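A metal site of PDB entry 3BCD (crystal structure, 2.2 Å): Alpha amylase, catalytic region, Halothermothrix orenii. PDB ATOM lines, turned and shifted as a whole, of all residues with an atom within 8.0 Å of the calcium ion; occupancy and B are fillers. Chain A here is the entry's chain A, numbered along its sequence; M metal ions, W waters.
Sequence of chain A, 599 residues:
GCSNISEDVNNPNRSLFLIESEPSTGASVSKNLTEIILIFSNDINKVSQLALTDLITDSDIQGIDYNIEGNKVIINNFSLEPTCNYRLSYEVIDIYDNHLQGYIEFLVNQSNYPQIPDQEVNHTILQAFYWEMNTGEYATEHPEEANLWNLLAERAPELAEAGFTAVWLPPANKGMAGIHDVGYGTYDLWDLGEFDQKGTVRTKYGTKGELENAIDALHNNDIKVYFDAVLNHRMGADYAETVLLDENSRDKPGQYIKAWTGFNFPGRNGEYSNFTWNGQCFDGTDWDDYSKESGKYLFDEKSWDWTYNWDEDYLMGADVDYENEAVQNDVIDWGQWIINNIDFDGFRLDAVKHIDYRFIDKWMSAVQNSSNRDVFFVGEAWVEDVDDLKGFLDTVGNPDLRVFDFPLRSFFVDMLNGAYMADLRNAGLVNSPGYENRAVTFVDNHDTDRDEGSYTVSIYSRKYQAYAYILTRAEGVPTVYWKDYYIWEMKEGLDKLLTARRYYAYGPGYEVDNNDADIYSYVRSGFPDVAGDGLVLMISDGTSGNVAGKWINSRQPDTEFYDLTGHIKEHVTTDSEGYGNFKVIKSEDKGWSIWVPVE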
ATOM      1  N   CYS A 281      17.228 -15.885 -27.068  1.00  0.00           N
ATOM      2  CA  CYS A 281      18.251 -16.031 -28.141  1.00  0.00           C
ATOM      3  C   CYS A 281      18.524 -14.777 -28.951  1.00  0.00           C
ATOM      4  O   CYS A 281      19.346 -14.795 -29.878  1.00  0.00           O
ATOM      5  CB  CYS A 281      17.825 -17.095 -29.142  1.00  0.00           C
ATOM      6  SG  CYS A 281      17.594 -18.753 -28.420  1.00  0.00           S
ATOM      7  N   PHE A 282      17.792 -13.711 -28.628  1.00  0.00           N
ATOM      8  CA  PHE A 282      17.828 -12.438 -29.378  1.00  0.00           C
ATOM      9  C   PHE A 282      18.014 -11.274 -28.382  1.00  0.00           C
ATOM     10  O   PHE A 282      17.583 -11.368 -27.233  1.00  0.00           O
ATOM     11  CB  PHE A 282      16.506 -12.198 -30.176  1.00  0.00           C
ATOM     12  CG  PHE A 282      16.122 -13.327 -31.138  1.00  0.00           C
ATOM     13  CD1 PHE A 282      15.014 -14.147 -30.879  1.00  0.00           C
ATOM     14  CD2 PHE A 282      16.848 -13.561 -32.309  1.00  0.00           C
ATOM     15  CE1 PHE A 282      14.685 -15.180 -31.754  1.00  0.00           C
ATOM     16  CE2 PHE A 282      16.540 -14.565 -33.176  1.00  0.00           C
ATOM     17  CZ  PHE A 282      15.453 -15.391 -32.909  1.00  0.00           C
ATOM     18  N   ASP A 283      18.643 -10.203 -28.847  1.00  0.00           N
ATOM     19  CA  ASP A 283      18.856  -8.965 -28.118  1.00  0.00           C
ATOM     20  C   ASP A 283      17.624  -8.060 -28.335  1.00  0.00           C
ATOM     21  O   ASP A 283      17.247  -7.261 -27.494  1.00  0.00           O
ATOM     22  CB  ASP A 283      20.097  -8.243 -28.683  1.00  0.00           C
ATOM     23  CG  ASP A 283      21.450  -8.806 -28.159  1.00  0.00           C
ATOM     24  OD1 ASP A 283      21.535  -9.283 -27.020  1.00  0.00           O
ATOM     25  OD2 ASP A 283      22.474  -8.753 -28.887  1.00  0.00           O
ATOM     26  N   GLY A 284      17.001  -8.159 -29.485  1.00  0.00           N
ATOM     27  CA  GLY A 284      15.769  -7.418 -29.659  1.00  0.00           C
ATOM     28  C   GLY A 284      15.114  -7.626 -31.017  1.00  0.00           C
ATOM     29  O   GLY A 284      15.534  -8.477 -31.786  1.00  0.00           O
ATOM     30  N   LEU A 298      14.998  -3.101 -27.401  1.00  0.00           N
ATOM     31  CA  LEU A 298      16.015  -3.922 -26.726  1.00  0.00           C
ATOM     32  C   LEU A 298      15.316  -4.698 -25.577  1.00  0.00           C
ATOM     33  O   LEU A 298      14.469  -4.129 -24.863  1.00  0.00           O
ATOM     34  CB  LEU A 298      17.146  -3.056 -26.175  1.00  0.00           C
ATOM     35  CG  LEU A 298      18.275  -3.833 -25.485  1.00  0.00           C
ATOM     36  CD1 LEU A 298      19.033  -4.662 -26.486  1.00  0.00           C
ATOM     37  CD2 LEU A 298      19.225  -2.921 -24.759  1.00  0.00           C
ATOM     38  N   GLU A 301      17.589  -7.029 -19.755  1.00  0.00           N
ATOM     39  CA  GLU A 301      18.869  -7.634 -19.465  1.00  0.00           C
ATOM     40  C   GLU A 301      19.752  -8.025 -20.666  1.00  0.00           C
ATOM     41  O   GLU A 301      20.839  -8.578 -20.453  1.00  0.00           O
ATOM     42  CB  GLU A 301      18.695  -8.839 -18.504  1.00  0.00           C
ATOM     43  CG  GLU A 301      18.276  -8.462 -17.052  1.00  0.00           C
ATOM     44  CD  GLU A 301      17.844  -9.706 -16.228  1.00  0.00           C
ATOM     45  OE1 GLU A 301      17.448  -9.534 -15.043  1.00  0.00           O
ATOM     46  OE2 GLU A 301      17.883 -10.864 -16.755  1.00  0.00           O
ATOM     47  N   LYS A 302      19.309  -7.794 -21.899  1.00  0.00           N
ATOM     48  CA  LYS A 302      20.156  -8.057 -23.071  1.00  0.00           C
ATOM     49  C   LYS A 302      20.966  -6.811 -23.362  1.00  0.00           C
ATOM     50  O   LYS A 302      20.571  -5.713 -22.934  1.00  0.00           O
ATOM     51  CB  LYS A 302      19.344  -8.404 -24.324  1.00  0.00           C
ATOM     52  CG  LYS A 302      18.600  -9.721 -24.269  1.00  0.00           C
ATOM     53  CD  LYS A 302      19.583 -10.879 -23.984  1.00  0.00           C
ATOM     54  CE  LYS A 302      18.882 -12.223 -24.070  1.00  0.00           C
ATOM     55  NZ  LYS A 302      19.824 -13.257 -24.576  1.00  0.00           N
ATOM     56  N   SER A 303      22.088  -6.956 -24.074  1.00  0.00           N
ATOM     57  CA  SER A 303      22.764  -5.798 -24.615  1.00  0.00           C
ATOM     58  C   SER A 303      23.256  -6.002 -26.059  1.00  0.00           C
ATOM     59  O   SER A 303      23.499  -7.156 -26.519  1.00  0.00           O
ATOM     60  CB  SER A 303      23.881  -5.294 -23.681  1.00  0.00           C
ATOM     61  OG  SER A 303      24.847  -6.297 -23.373  1.00  0.00           O
ATOM     62  N   TRP A 304      23.309  -4.926 -26.824  1.00  0.00           N
ATOM     63  CA  TRP A 304      23.747  -5.034 -28.174  1.00  0.00           C
ATOM     64  C   TRP A 304      25.183  -5.505 -28.176  1.00  0.00           C
ATOM     65  O   TRP A 304      25.966  -5.151 -27.282  1.00  0.00           O
ATOM     66  CB  TRP A 304      23.636  -3.686 -28.865  1.00  0.00           C
ATOM     67  CG  TRP A 304      22.247  -3.114 -28.942  1.00  0.00           C
ATOM     68  CD1 TRP A 304      21.893  -1.889 -28.524  1.00  0.00           C
ATOM     69  CD2 TRP A 304      21.077  -3.685 -29.530  1.00  0.00           C
ATOM     70  NE1 TRP A 304      20.570  -1.651 -28.775  1.00  0.00           N
ATOM     71  CE2 TRP A 304      20.035  -2.756 -29.374  1.00  0.00           C
ATOM     72  CE3 TRP A 304      20.799  -4.926 -30.162  1.00  0.00           C
ATOM     73  CZ2 TRP A 304      18.705  -3.003 -29.839  1.00  0.00           C
ATOM     74  CZ3 TRP A 304      19.512  -5.185 -30.577  1.00  0.00           C
ATOM     75  CH2 TRP A 304      18.459  -4.217 -30.441  1.00  0.00           C
ATOM     76  N   ASP A 305      25.551  -6.273 -29.202  1.00  0.00           N
ATOM     77  CA  ASP A 305      26.861  -6.907 -29.274  1.00  0.00           C
ATOM     78  C   ASP A 305      27.869  -5.953 -29.754  1.00  0.00           C
ATOM     79  O   ASP A 305      27.532  -4.901 -30.299  1.00  0.00           O
ATOM     80  CB  ASP A 305      26.792  -8.166 -30.123  1.00  0.00           C
ATOM     81  CG  ASP A 305      25.653  -9.128 -29.656  1.00  0.00           C
ATOM     82  OD1 ASP A 305      25.507  -9.216 -28.431  1.00  0.00           O
ATOM     83  OD2 ASP A 305      24.921  -9.778 -30.478  1.00  0.00           O
ATOM     84  N   TRP A 306      29.132  -6.222 -29.472  1.00  0.00           N
ATOM     85  CA  TRP A 306      30.173  -5.298 -29.876  1.00  0.00           C
ATOM     86  C   TRP A 306      30.325  -5.253 -31.375  1.00  0.00           C
ATOM     87  O   TRP A 306      30.591  -6.235 -31.997  1.00  0.00           O
ATOM     88  CB  TRP A 306      31.516  -5.613 -29.217  1.00  0.00           C
ATOM     89  CG  TRP A 306      31.577  -5.564 -27.711  1.00  0.00           C
ATOM     90  CD1 TRP A 306      30.543  -5.459 -26.824  1.00  0.00           C
ATOM     91  CD2 TRP A 306      32.757  -5.730 -26.940  1.00  0.00           C
ATOM     92  NE1 TRP A 306      31.020  -5.539 -25.548  1.00  0.00           N
ATOM     93  CE2 TRP A 306      32.378  -5.716 -25.597  1.00  0.00           C
ATOM     94  CE3 TRP A 306      34.109  -5.929 -27.273  1.00  0.00           C
ATOM     95  CZ2 TRP A 306      33.291  -5.858 -24.579  1.00  0.00           C
ATOM     96  CZ3 TRP A 306      35.022  -6.059 -26.271  1.00  0.00           C
ATOM     97  CH2 TRP A 306      34.623  -6.010 -24.927  1.00  0.00           C
ATOM     98  N   ASP A 313      24.526  -2.913 -34.169  1.00  0.00           N
ATOM     99  CA  ASP A 313      24.123  -4.316 -34.103  1.00  0.00           C
ATOM    100  C   ASP A 313      22.690  -4.406 -34.662  1.00  0.00           C
ATOM    101  O   ASP A 313      22.380  -5.343 -35.397  1.00  0.00           O
ATOM    102  CB  ASP A 313      24.263  -4.846 -32.662  1.00  0.00           C
ATOM    103  CG  ASP A 313      23.992  -6.371 -32.516  1.00  0.00           C
ATOM    104  OD1 ASP A 313      24.083  -7.215 -33.448  1.00  0.00           O
ATOM    105  OD2 ASP A 313      23.707  -6.741 -31.383  1.00  0.00           O
ATOM    106  N   ASP A 319      16.867  -9.692 -33.763  1.00  0.00           N
ATOM    107  CA  ASP A 319      18.375  -9.570 -33.868  1.00  0.00           C
ATOM    108  C   ASP A 319      18.998 -10.640 -33.019  1.00  0.00           C
ATOM    109  O   ASP A 319      18.604 -10.792 -31.912  1.00  0.00           O
ATOM    110  CB  ASP A 319      18.879  -8.247 -33.336  1.00  0.00           C
ATOM    111  CG  ASP A 319      20.425  -8.058 -33.505  1.00  0.00           C
ATOM    112  OD1 ASP A 319      20.778  -7.694 -34.669  1.00  0.00           O
ATOM    113  OD2 ASP A 319      21.239  -8.185 -32.484  1.00  0.00           O
ATOM    114  N   VAL A 320      19.985 -11.365 -33.518  1.00  0.00           N
ATOM    115  CA  VAL A 320      20.521 -12.512 -32.779  1.00  0.00           C
ATOM    116  C   VAL A 320      21.436 -12.056 -31.674  1.00  0.00           C
ATOM    117  O   VAL A 320      22.179 -11.113 -31.856  1.00  0.00           O
ATOM    118  CB  VAL A 320      21.312 -13.484 -33.698  1.00  0.00           C
ATOM    119  CG1 VAL A 320      21.972 -14.642 -32.899  1.00  0.00           C
ATOM    120  CG2 VAL A 320      20.427 -14.032 -34.795  1.00  0.00           C
ATOM    121  N   ASP A 321      21.408 -12.748 -30.533  1.00  0.00           N
ATOM    122  CA  ASP A 321      22.281 -12.416 -29.439  1.00  0.00           C
ATOM    123  C   ASP A 321      23.490 -13.310 -29.481  1.00  0.00           C
ATOM    124  O   ASP A 321      23.381 -14.441 -29.020  1.00  0.00           O
ATOM    125  CB  ASP A 321      21.550 -12.537 -28.089  1.00  0.00           C
ATOM    126  CG  ASP A 321      22.480 -12.231 -26.857  1.00  0.00           C
ATOM    127  OD1 ASP A 321      23.589 -11.662 -27.035  1.00  0.00           O
ATOM    128  OD2 ASP A 321      22.095 -12.593 -25.727  1.00  0.00           O
ATOM    129  N   TYR A 322      24.620 -12.826 -30.012  1.00  0.00           N
ATOM    130  CA  TYR A 322      25.859 -13.634 -30.057  1.00  0.00           C
ATOM    131  C   TYR A 322      26.669 -13.655 -28.766  1.00  0.00           C
ATOM    132  O   TYR A 322      27.755 -14.260 -28.724  1.00  0.00           O
ATOM    133  CB  TYR A 322      26.729 -13.292 -31.296  1.00  0.00           C
ATOM    134  CG  TYR A 322      26.117 -13.906 -32.512  1.00  0.00           C
ATOM    135  CD1 TYR A 322      25.514 -13.125 -33.490  1.00  0.00           C
ATOM    136  CD2 TYR A 322      26.005 -15.298 -32.622  1.00  0.00           C
ATOM    137  CE1 TYR A 322      24.877 -13.732 -34.591  1.00  0.00           C
ATOM    138  CE2 TYR A 322      25.360 -15.905 -33.686  1.00  0.00           C
ATOM    139  CZ  TYR A 322      24.787 -15.125 -34.665  1.00  0.00           C
ATOM    140  OH  TYR A 322      24.162 -15.735 -35.744  1.00  0.00           O
ATOM    141  N   GLU A 323      26.151 -13.038 -27.705  1.00  0.00           N
ATOM    142  CA  GLU A 323      26.690 -13.286 -26.366  1.00  0.00           C
ATOM    143  C   GLU A 323      26.105 -14.566 -25.779  1.00  0.00           C
ATOM    144  O   GLU A 323      26.668 -15.118 -24.847  1.00  0.00           O
ATOM    145  CB  GLU A 323      26.523 -12.056 -25.442  1.00  0.00           C
ATOM    146  CG  GLU A 323      27.485 -10.901 -25.876  1.00  0.00           C
ATOM    147  CD  GLU A 323      27.019  -9.472 -25.532  1.00  0.00           C
ATOM    148  OE1 GLU A 323      25.785  -9.236 -25.435  1.00  0.00           O
ATOM    149  OE2 GLU A 323      27.919  -8.610 -25.363  1.00  0.00           O
ATOM    150  N   ASN A 324      24.997 -15.055 -26.350  1.00  0.00           N
ATOM    151  CA  ASN A 324      24.354 -16.328 -25.927  1.00  0.00           C
ATOM    152  C   ASN A 324      25.094 -17.610 -26.413  1.00  0.00           C
ATOM    153  O   ASN A 324      25.108 -17.915 -27.589  1.00  0.00           O
ATOM    154  CB  ASN A 324      22.831 -16.379 -26.308  1.00  0.00           C
ATOM    155  CG  ASN A 324      22.189 -17.719 -26.017  1.00  0.00           C
ATOM    156  OD1 ASN A 324      22.851 -18.737 -26.158  1.00  0.00           O
ATOM    157  ND2 ASN A 324      20.888 -17.746 -25.624  1.00  0.00           N
ATOM    158  N   ASP A 356      28.329  -9.118 -33.986  1.00  0.00           N
ATOM    159  CA  ASP A 356      29.352  -9.172 -32.997  1.00  0.00           C
ATOM    160  C   ASP A 356      30.697  -9.558 -33.605  1.00  0.00           C
ATOM    161  O   ASP A 356      30.873 -10.659 -34.014  1.00  0.00           O
ATOM    162  CB  ASP A 356      28.913 -10.201 -31.974  1.00  0.00           C
ATOM    163  CG  ASP A 356      29.742 -10.152 -30.697  1.00  0.00           C
ATOM    164  OD1 ASP A 356      30.980 -10.224 -30.766  1.00  0.00           O
ATOM    165  OD2 ASP A 356      29.140 -10.117 -29.598  1.00  0.00           O
ATOM    166  N   ARG A 358      33.347 -10.430 -32.356  1.00  0.00           N
ATOM    167  CA  ARG A 358      34.098 -11.417 -31.565  1.00  0.00           C
ATOM    168  C   ARG A 358      33.616 -12.725 -32.051  1.00  0.00           C
ATOM    169  O   ARG A 358      34.398 -13.628 -32.226  1.00  0.00           O
ATOM    170  CB  ARG A 358      33.818 -11.339 -30.059  1.00  0.00           C
ATOM    171  CG  ARG A 358      34.352 -10.089 -29.336  1.00  0.00           C
ATOM    172  CD  ARG A 358      33.627  -9.864 -27.940  1.00  0.00           C
ATOM    173  NE  ARG A 358      32.185  -9.570 -28.000  1.00  0.00           N
ATOM    174  CZ  ARG A 358      31.433  -9.230 -26.963  1.00  0.00           C
ATOM    175  NH1 ARG A 358      31.986  -9.164 -25.796  1.00  0.00           N
ATOM    176  NH2 ARG A 358      30.148  -8.934 -27.089  1.00  0.00           N
HETATM  177 CA    CA M   1      23.898  -9.395 -26.813  1.00  0.00          CA
HETATM  178  O   HOH W   1      22.668  -9.644 -24.628  1.00  0.00           O
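OD2 of Asp 305 sits at hydrogen-bond distance from N of Tyr 322.
The side-chain carboxylate (OD2) of Asp 313 is in hydrogen-bond range of the backbone NH (N) of Asp 305 (2.9 Å).
The side-chain carboxylate (OD2) of Asp 321 lies within salt-bridge range of the side-chain amino group (NZ) of Lys 302, 2.6 Å away.
O of Cys 281 lies within hydrogen-bond range of N of Asp 321, at 3.0 Å.
The guanidinium group (NH2) of Arg 358 lies within salt-bridge range of the side-chain carboxylate (OE2) of Glu 323.
O of Asp 319 sits at hydrogen-bond distance from N of Asp 283 (3.1 Å).
Five residues have an atom within 4 Å of the calcium ion: Asp 283, Ser 303, Asp 305, Asp 321 and Glu 323.
The nearest printed residue that does not touch the calcium ion is Trp 304 (4.3 Å).
The calcium ion is bound by OD1 of Asp 305 (2.3 Å).
O of Ser 303 binds the calcium ion (2.3 Å).
The calcium ion is bound by the side-chain carboxylate (OD1) of Asp 321 (2.3 Å).
The calcium ion is bound by OE1 of Glu 323, at 2.3 Å.
The calcium ion is bound by OD1 of Asp 283 (2.4 Å).
Water W1 is bound to the calcium ion (2.5 Å).
The side-chain carboxylate (OD2) of Asp 283 binds the calcium ion (2.6 Å).
Water W1 lies within hydrogen-bond range of the backbone NH (N) of Ser 303 (2.8 Å) and the side-chain carboxylate (OD2) of Asp 321 (3.2 Å).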
